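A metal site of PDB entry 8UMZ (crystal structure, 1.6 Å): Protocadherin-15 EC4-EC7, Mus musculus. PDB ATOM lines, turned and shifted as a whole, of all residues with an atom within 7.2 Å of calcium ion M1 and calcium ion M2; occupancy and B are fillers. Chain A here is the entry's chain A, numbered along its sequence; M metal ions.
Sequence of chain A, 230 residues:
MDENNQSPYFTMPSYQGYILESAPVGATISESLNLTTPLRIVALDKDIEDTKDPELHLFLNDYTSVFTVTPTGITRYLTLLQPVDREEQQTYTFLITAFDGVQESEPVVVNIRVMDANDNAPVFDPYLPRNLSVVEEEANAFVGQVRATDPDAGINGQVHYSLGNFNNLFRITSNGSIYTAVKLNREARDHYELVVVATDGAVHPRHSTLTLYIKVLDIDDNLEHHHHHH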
ATOM      1  N   GLU A  21       5.916 -16.674   5.444  1.00  0.00           N
ATOM      2  CA  GLU A  21       4.783 -17.513   5.795  1.00  0.00           C
ATOM      3  C   GLU A  21       4.551 -17.534   7.321  1.00  0.00           C
ATOM      4  O   GLU A  21       3.454 -17.801   7.780  1.00  0.00           O
ATOM      5  CB  GLU A  21       4.917 -18.971   5.331  1.00  0.00           C
ATOM      6  CG  GLU A  21       6.130 -19.743   5.885  1.00  0.00           C
ATOM      7  CD  GLU A  21       6.187 -21.115   5.252  1.00  0.00           C
ATOM      8  OE1 GLU A  21       5.160 -21.692   5.077  1.00  0.00           O
ATOM      9  OE2 GLU A  21       7.335 -21.673   5.002  1.00  0.00           O
ATOM     10  N   ASP A  85       0.785 -20.443   4.090  1.00  0.00           N
ATOM     11  CA  ASP A  85       1.668 -21.597   4.156  1.00  0.00           C
ATOM     12  C   ASP A  85       2.302 -21.796   2.800  1.00  0.00           C
ATOM     13  O   ASP A  85       1.621 -22.147   1.851  1.00  0.00           O
ATOM     14  CB  ASP A  85       0.854 -22.802   4.640  1.00  0.00           C
ATOM     15  CG  ASP A  85       1.654 -24.100   4.647  1.00  0.00           C
ATOM     16  OD1 ASP A  85       2.868 -24.026   4.606  1.00  0.00           O
ATOM     17  OD2 ASP A  85       1.061 -25.139   4.701  1.00  0.00           O
ATOM     18  N   ARG A  86       3.650 -21.737   2.743  1.00  0.00           N
ATOM     19  CA  ARG A  86       4.325 -21.781   1.483  1.00  0.00           C
ATOM     20  C   ARG A  86       4.216 -23.209   0.954  1.00  0.00           C
ATOM     21  O   ARG A  86       4.139 -23.394  -0.245  1.00  0.00           O
ATOM     22  CB  ARG A  86       5.755 -21.270   1.639  1.00  0.00           C
ATOM     23  CG  ARG A  86       6.438 -21.093   0.291  1.00  0.00           C
ATOM     24  CD  ARG A  86       7.918 -21.318   0.468  1.00  0.00           C
ATOM     25  NE  ARG A  86       8.206 -22.707   0.789  1.00  0.00           N
ATOM     26  CZ  ARG A  86       8.156 -23.731  -0.058  1.00  0.00           C
ATOM     27  NH1 ARG A  86       7.844 -23.559  -1.329  1.00  0.00           N
ATOM     28  NH2 ARG A  86       8.457 -24.941   0.384  1.00  0.00           N
ATOM     29  N   GLU A  87       4.102 -24.194   1.866  1.00  0.00           N
ATOM     30  CA  GLU A  87       4.078 -25.581   1.427  1.00  0.00           C
ATOM     31  C   GLU A  87       2.694 -25.949   0.856  1.00  0.00           C
ATOM     32  O   GLU A  87       2.559 -26.967   0.182  1.00  0.00           O
ATOM     33  CB  GLU A  87       4.415 -26.506   2.593  1.00  0.00           C
ATOM     34  CG  GLU A  87       5.906 -26.583   2.907  1.00  0.00           C
ATOM     35  CD  GLU A  87       6.544 -25.357   3.524  1.00  0.00           C
ATOM     36  OE1 GLU A  87       6.083 -24.928   4.593  1.00  0.00           O
ATOM     37  OE2 GLU A  87       7.560 -24.854   2.948  1.00  0.00           O
ATOM     38  N   MET A 115       7.233 -16.042   1.138  1.00  0.00           N
ATOM     39  CA  MET A 115       8.625 -16.426   1.340  1.00  0.00           C
ATOM     40  C   MET A 115       8.692 -17.595   2.311  1.00  0.00           C
ATOM     41  O   MET A 115       7.838 -17.758   3.179  1.00  0.00           O
ATOM     42  CB  MET A 115       9.496 -15.284   1.855  1.00  0.00           C
ATOM     43  CG  MET A 115       9.471 -14.013   1.017  1.00  0.00           C
ATOM     44  SD  MET A 115       9.993 -14.265  -0.688  1.00  0.00           S
ATOM     45  CE  MET A 115      11.764 -14.459  -0.448  1.00  0.00           C
ATOM     46  N   ASP A 116       9.703 -18.448   2.135  1.00  0.00           N
ATOM     47  CA  ASP A 116       9.821 -19.630   2.961  1.00  0.00           C
ATOM     48  C   ASP A 116      10.464 -19.306   4.291  1.00  0.00           C
ATOM     49  O   ASP A 116      11.490 -18.624   4.413  1.00  0.00           O
ATOM     50  CB  ASP A 116      10.634 -20.672   2.197  1.00  0.00           C
ATOM     51  CG  ASP A 116      10.674 -22.005   2.910  1.00  0.00           C
ATOM     52  OD1 ASP A 116       9.621 -22.513   3.244  1.00  0.00           O
ATOM     53  OD2 ASP A 116      11.822 -22.544   3.064  1.00  0.00           O
ATOM     54  N   ALA A 117       9.858 -19.860   5.332  1.00  0.00           N
ATOM     55  CA  ALA A 117      10.452 -19.930   6.638  1.00  0.00           C
ATOM     56  C   ALA A 117      10.957 -21.372   6.787  1.00  0.00           C
ATOM     57  O   ALA A 117      10.381 -22.294   6.219  1.00  0.00           O
ATOM     58  CB  ALA A 117       9.411 -19.638   7.693  1.00  0.00           C
ATOM     59  N   ASN A 118      12.021 -21.552   7.565  1.00  0.00           N
ATOM     60  CA  ASN A 118      12.397 -22.899   7.966  1.00  0.00           C
ATOM     61  C   ASN A 118      11.524 -23.385   9.114  1.00  0.00           C
ATOM     62  O   ASN A 118      12.019 -23.496  10.246  1.00  0.00           O
ATOM     63  CB  ASN A 118      13.877 -22.990   8.329  1.00  0.00           C
ATOM     64  CG  ASN A 118      14.220 -24.441   8.466  1.00  0.00           C
ATOM     65  OD1 ASN A 118      13.678 -25.256   7.729  1.00  0.00           O
ATOM     66  ND2 ASN A 118      15.003 -24.758   9.493  1.00  0.00           N
ATOM     67  N   ASP A 119      10.263 -23.714   8.807  1.00  0.00           N
ATOM     68  CA  ASP A 119       9.191 -23.993   9.767  1.00  0.00           C
ATOM     69  C   ASP A 119       8.901 -25.490   9.901  1.00  0.00           C
ATOM     70  O   ASP A 119       7.980 -25.931  10.608  1.00  0.00           O
ATOM     71  CB  ASP A 119       7.935 -23.141   9.483  1.00  0.00           C
ATOM     72  CG  ASP A 119       7.242 -23.321   8.139  1.00  0.00           C
ATOM     73  OD1 ASP A 119       7.892 -23.835   7.215  1.00  0.00           O
ATOM     74  OD2 ASP A 119       5.981 -23.008   8.011  1.00  0.00           O
ATOM     75  N   ASN A 120       9.730 -26.310   9.241  1.00  0.00           N
ATOM     76  CA  ASN A 120       9.551 -27.750   9.267  1.00  0.00           C
ATOM     77  C   ASN A 120      10.894 -28.377   9.646  1.00  0.00           C
ATOM     78  O   ASN A 120      11.942 -27.944   9.165  1.00  0.00           O
ATOM     79  CB  ASN A 120       9.001 -28.354   7.976  1.00  0.00           C
ATOM     80  CG  ASN A 120       7.588 -27.888   7.698  1.00  0.00           C
ATOM     81  OD1 ASN A 120       7.395 -26.881   7.034  1.00  0.00           O
ATOM     82  ND2 ASN A 120       6.626 -28.688   8.102  1.00  0.00           N
ATOM     83  N   ALA A 121      10.829 -29.381  10.512  1.00  0.00           N
ATOM     84  CA  ALA A 121      11.955 -30.264  10.730  1.00  0.00           C
ATOM     85  C   ALA A 121      11.886 -31.416   9.735  1.00  0.00           C
ATOM     86  O   ALA A 121      10.826 -31.780   9.261  1.00  0.00           O
ATOM     87  CB  ALA A 121      11.955 -30.757  12.166  1.00  0.00           C
ATOM     88  N   PRO A 122      13.010 -32.119   9.442  1.00  0.00           N
ATOM     89  CA  PRO A 122      12.934 -33.345   8.667  1.00  0.00           C
ATOM     90  C   PRO A 122      12.001 -34.338   9.370  1.00  0.00           C
ATOM     91  O   PRO A 122      11.962 -34.431  10.597  1.00  0.00           O
ATOM     92  CB  PRO A 122      14.409 -33.817   8.684  1.00  0.00           C
ATOM     93  CG  PRO A 122      15.193 -32.566   8.771  1.00  0.00           C
ATOM     94  CD  PRO A 122      14.404 -31.746   9.762  1.00  0.00           C
ATOM     95  N   ASP A 150      12.046 -33.219   4.108  1.00  0.00           N
ATOM     96  CA  ASP A 150      11.740 -31.932   4.701  1.00  0.00           C
ATOM     97  C   ASP A 150      11.079 -31.122   3.611  1.00  0.00           C
ATOM     98  O   ASP A 150      11.694 -30.882   2.563  1.00  0.00           O
ATOM     99  CB  ASP A 150      13.048 -31.287   5.152  1.00  0.00           C
ATOM    100  CG  ASP A 150      12.927 -30.007   5.965  1.00  0.00           C
ATOM    101  OD1 ASP A 150      12.116 -29.109   5.585  1.00  0.00           O
ATOM    102  OD2 ASP A 150      13.626 -29.899   6.956  1.00  0.00           O
ATOM    103  N   PRO A 151       9.834 -30.651   3.836  1.00  0.00           N
ATOM    104  CA  PRO A 151       9.056 -30.016   2.766  1.00  0.00           C
ATOM    105  C   PRO A 151       9.465 -28.552   2.517  1.00  0.00           C
ATOM    106  O   PRO A 151       8.908 -27.953   1.558  1.00  0.00           O
ATOM    107  CB  PRO A 151       7.615 -30.188   3.299  1.00  0.00           C
ATOM    108  CG  PRO A 151       7.775 -30.023   4.791  1.00  0.00           C
ATOM    109  CD  PRO A 151       9.131 -30.645   5.121  1.00  0.00           C
ATOM    110  N   ASP A 152      10.355 -27.942   3.345  1.00  0.00           N
ATOM    111  CA  ASP A 152      10.756 -26.554   3.137  1.00  0.00           C
ATOM    112  C   ASP A 152      11.583 -26.395   1.867  1.00  0.00           C
ATOM    113  O   ASP A 152      11.914 -27.380   1.217  1.00  0.00           O
ATOM    114  CB  ASP A 152      11.492 -25.930   4.319  1.00  0.00           C
ATOM    115  CG  ASP A 152      10.743 -25.994   5.628  1.00  0.00           C
ATOM    116  OD1 ASP A 152       9.626 -25.510   5.659  1.00  0.00           O
ATOM    117  OD2 ASP A 152      11.369 -26.349   6.643  1.00  0.00           O
ATOM    118  N   ALA A 153      11.884 -25.140   1.516  1.00  0.00           N
ATOM    119  CA  ALA A 153      12.509 -24.796   0.254  1.00  0.00           C
ATOM    120  C   ALA A 153      14.020 -24.696   0.379  1.00  0.00           C
ATOM    121  O   ALA A 153      14.576 -24.165   1.340  1.00  0.00           O
ATOM    122  CB  ALA A 153      11.978 -23.453  -0.222  1.00  0.00           C
ATOM    123  N   ILE A 155      17.705 -24.847   0.904  1.00  0.00           N
ATOM    124  CA  ILE A 155      18.584 -25.411   1.953  1.00  0.00           C
ATOM    125  C   ILE A 155      17.730 -25.775   3.160  1.00  0.00           C
ATOM    126  O   ILE A 155      18.009 -26.730   3.905  1.00  0.00           O
ATOM    127  CB  ILE A 155      19.695 -24.465   2.386  1.00  0.00           C
ATOM    128  CG1 ILE A 155      19.124 -23.145   2.981  1.00  0.00           C
ATOM    129  CG2 ILE A 155      20.713 -24.220   1.318  1.00  0.00           C
ATOM    130  CD1 ILE A 155      20.204 -22.114   3.245  1.00  0.00           C
ATOM    131  N   ASN A 156      16.585 -25.088   3.317  1.00  0.00           N
ATOM    132  CA  ASN A 156      15.718 -25.359   4.453  1.00  0.00           C
ATOM    133  C   ASN A 156      15.080 -26.755   4.347  1.00  0.00           C
ATOM    134  O   ASN A 156      14.589 -27.224   5.354  1.00  0.00           O
ATOM    135  CB  ASN A 156      14.655 -24.252   4.630  1.00  0.00           C
ATOM    136  CG  ASN A 156      15.194 -22.858   4.823  1.00  0.00           C
ATOM    137  OD1 ASN A 156      16.325 -22.654   5.296  1.00  0.00           O
ATOM    138  ND2 ASN A 156      14.376 -21.850   4.466  1.00  0.00           N
ATOM    139  N   GLY A 157      15.059 -27.368   3.148  1.00  0.00           N
ATOM    140  CA  GLY A 157      14.480 -28.673   2.894  1.00  0.00           C
ATOM    141  C   GLY A 157      15.542 -29.733   2.567  1.00  0.00           C
ATOM    142  O   GLY A 157      15.154 -30.862   2.348  1.00  0.00           O
ATOM    143  N   GLN A 158      16.838 -29.384   2.614  1.00  0.00           N
ATOM    144  CA  GLN A 158      17.905 -30.365   2.367  1.00  0.00           C
ATOM    145  C   GLN A 158      18.339 -31.024   3.661  1.00  0.00           C
ATOM    146  O   GLN A 158      18.503 -30.386   4.697  1.00  0.00           O
ATOM    147  CB  GLN A 158      19.065 -29.744   1.620  1.00  0.00           C
ATOM    148  CG  GLN A 158      18.700 -29.391   0.193  1.00  0.00           C
ATOM    149  CD  GLN A 158      19.761 -28.492  -0.396  1.00  0.00           C
ATOM    150  OE1 GLN A 158      20.906 -28.366   0.073  1.00  0.00           O
ATOM    151  NE2 GLN A 158      19.356 -27.760  -1.410  1.00  0.00           N
ATOM    152  N   THR A 199      19.139 -33.429  10.000  1.00  0.00           N
ATOM    153  CA  THR A 199      19.262 -31.970  10.195  1.00  0.00           C
ATOM    154  C   THR A 199      19.121 -31.303   8.828  1.00  0.00           C
ATOM    155  O   THR A 199      19.663 -31.752   7.829  1.00  0.00           O
ATOM    156  CB  THR A 199      20.615 -31.608  10.783  1.00  0.00           C
ATOM    157  OG1 THR A 199      20.834 -32.315  12.025  1.00  0.00           O
ATOM    158  CG2 THR A 199      20.791 -30.122  11.019  1.00  0.00           C
ATOM    159  N   ASP A 200      18.301 -30.248   8.734  1.00  0.00           N
ATOM    160  CA  ASP A 200      18.262 -29.508   7.481  1.00  0.00           C
ATOM    161  C   ASP A 200      19.449 -28.557   7.327  1.00  0.00           C
ATOM    162  O   ASP A 200      20.276 -28.390   8.220  1.00  0.00           O
ATOM    163  CB  ASP A 200      16.881 -28.868   7.309  1.00  0.00           C
ATOM    164  CG  ASP A 200      16.465 -27.871   8.378  1.00  0.00           C
ATOM    165  OD1 ASP A 200      17.349 -27.214   8.864  1.00  0.00           O
ATOM    166  OD2 ASP A 200      15.182 -27.756   8.658  1.00  0.00           O
ATOM    167  N   GLY A 201      19.513 -27.933   6.129  1.00  0.00           N
ATOM    168  CA  GLY A 201      20.563 -27.016   5.738  1.00  0.00           C
ATOM    169  C   GLY A 201      20.293 -25.545   6.062  1.00  0.00           C
ATOM    170  O   GLY A 201      21.077 -24.716   5.645  1.00  0.00           O
ATOM    171  N   ALA A 202      19.315 -25.209   6.884  1.00  0.00           N
ATOM    172  CA  ALA A 202      18.982 -23.817   7.133  1.00  0.00           C
ATOM    173  C   ALA A 202      20.081 -23.083   7.888  1.00  0.00           C
ATOM    174  O   ALA A 202      20.857 -23.672   8.651  1.00  0.00           O
ATOM    175  CB  ALA A 202      17.710 -23.766   7.889  1.00  0.00           C
ATOM    176  N   HIS A 204      19.341 -21.322  10.348  1.00  0.00           N
ATOM    177  CA  HIS A 204      18.890 -21.619  11.699  1.00  0.00           C
ATOM    178  C   HIS A 204      18.373 -23.055  11.633  1.00  0.00           C
ATOM    179  O   HIS A 204      17.196 -23.249  11.363  1.00  0.00           O
ATOM    180  CB  HIS A 204      17.833 -20.584  12.114  1.00  0.00           C
ATOM    181  CG  HIS A 204      18.296 -19.162  12.063  1.00  0.00           C
ATOM    182  ND1 HIS A 204      17.693 -18.203  11.266  1.00  0.00           N
ATOM    183  CD2 HIS A 204      19.285 -18.525  12.730  1.00  0.00           C
ATOM    184  CE1 HIS A 204      18.325 -17.037  11.459  1.00  0.00           C
ATOM    185  NE2 HIS A 204      19.260 -17.206  12.356  1.00  0.00           N
ATOM    186  N   PRO A 205      19.243 -24.090  11.710  1.00  0.00           N
ATOM    187  CA  PRO A 205      18.819 -25.453  11.342  1.00  0.00           C
ATOM    188  C   PRO A 205      17.749 -26.014  12.252  1.00  0.00           C
ATOM    189  O   PRO A 205      17.673 -25.641  13.427  1.00  0.00           O
ATOM    190  CB  PRO A 205      20.127 -26.244  11.436  1.00  0.00           C
ATOM    191  CG  PRO A 205      20.951 -25.440  12.405  1.00  0.00           C
ATOM    192  CD  PRO A 205      20.683 -24.019  11.942  1.00  0.00           C
ATOM    193  N   ARG A 206      16.951 -26.938  11.724  1.00  0.00           N
ATOM    194  CA  ARG A 206      16.036 -27.751  12.539  1.00  0.00           C
ATOM    195  C   ARG A 206      16.464 -29.211  12.370  1.00  0.00           C
ATOM    196  O   ARG A 206      17.051 -29.557  11.339  1.00  0.00           O
ATOM    197  CB  ARG A 206      14.574 -27.564  12.176  1.00  0.00           C
ATOM    198  CG  ARG A 206      13.972 -26.231  12.602  1.00  0.00           C
ATOM    199  CD  ARG A 206      12.498 -26.222  12.275  1.00  0.00           C
ATOM    200  NE  ARG A 206      11.789 -25.001  12.702  1.00  0.00           N
ATOM    201  CZ  ARG A 206      11.361 -24.789  13.956  1.00  0.00           C
ATOM    202  NH1 ARG A 206      11.599 -25.681  14.902  1.00  0.00           N
ATOM    203  NH2 ARG A 206      10.736 -23.660  14.287  1.00  0.00           N
HETATM  204 CA    CA M   1       8.547 -23.548   5.023  1.00  0.00          CA
HETATM  205 CA    CA M   2      13.271 -27.527   7.253  1.00  0.00          CA
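Calcium ion M1 is bound by the side-chain carboxylate (OE2) of Glu 21 (2.2 Å), the side-chain carboxylate (OD1) of Asp 119 (2.3 Å), the side-chain carboxylate (OD1) of Asp 116 (2.3 Å), the side-chain carboxylate (OD1) of Asp 152 (2.3 Å), the backbone carbonyl oxygen (O) of Ala 117 (2.5 Å), the side-chain carboxylate (OE2) of Glu 87 (2.6 Å) and the side-chain carboxylate (OE1) of Glu 87 (2.9 Å).
OE1 of Glu 21 lies within hydrogen-bond range of N of Arg 86 (2.8 Å).
N of Glu 21 lies within hydrogen-bond range of O of Met 115, at 3.2 Å.
OD1 of Asp 119 sits close to OD1 of Asn 120 (3.1 Å).
The side-chain amide nitrogen (ND2) of Asn 156 sits at hydrogen-bond distance from the side-chain carboxylate (OD2) of Asp 116, 3.0 Å away.
NE of Arg 206 is in hydrogen-bond range of O of Asn 118 (2.9 Å).
ND2 of Asn 118 sits at hydrogen-bond distance from O of His 204, 3.3 Å away.
The side-chain carboxylate (OE1) of Glu 87 sits close to the side-chain amide oxygen (OD1) of Asn 120, 3.4 Å away.
The guanidinium group (NH2) of Arg 86 sits close to the side-chain carboxylate (OE2) of Glu 87.
Six residues have an atom within 4 Å of calcium ion M2: Asn 118, Asn 120, Asp 150, Asp 152, Asn 156 and Asp 200.
The nearest printed residue that does not touch calcium ion M2 is Ala 121 (4.5 Å).
Within 4 Å of calcium ion M1: Glu 21, Glu 87, Asp 116, Ala 117, Asp 119 and Asp 152.
The nearest printed residue that does not touch calcium ion M1 is Asn 120 (4.1 Å).
Calcium ion M2 is bound by OD2 of Asp 152 (2.3 Å), O of Asn 156 (2.3 Å), OD1 of Asn 118 (2.4 Å), O of Asn 120 (2.4 Å), OD2 of Asp 200 (2.4 Å), OD2 of Asp 150 (2.4 Å) and OD1 of Asp 150 (2.6 Å).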
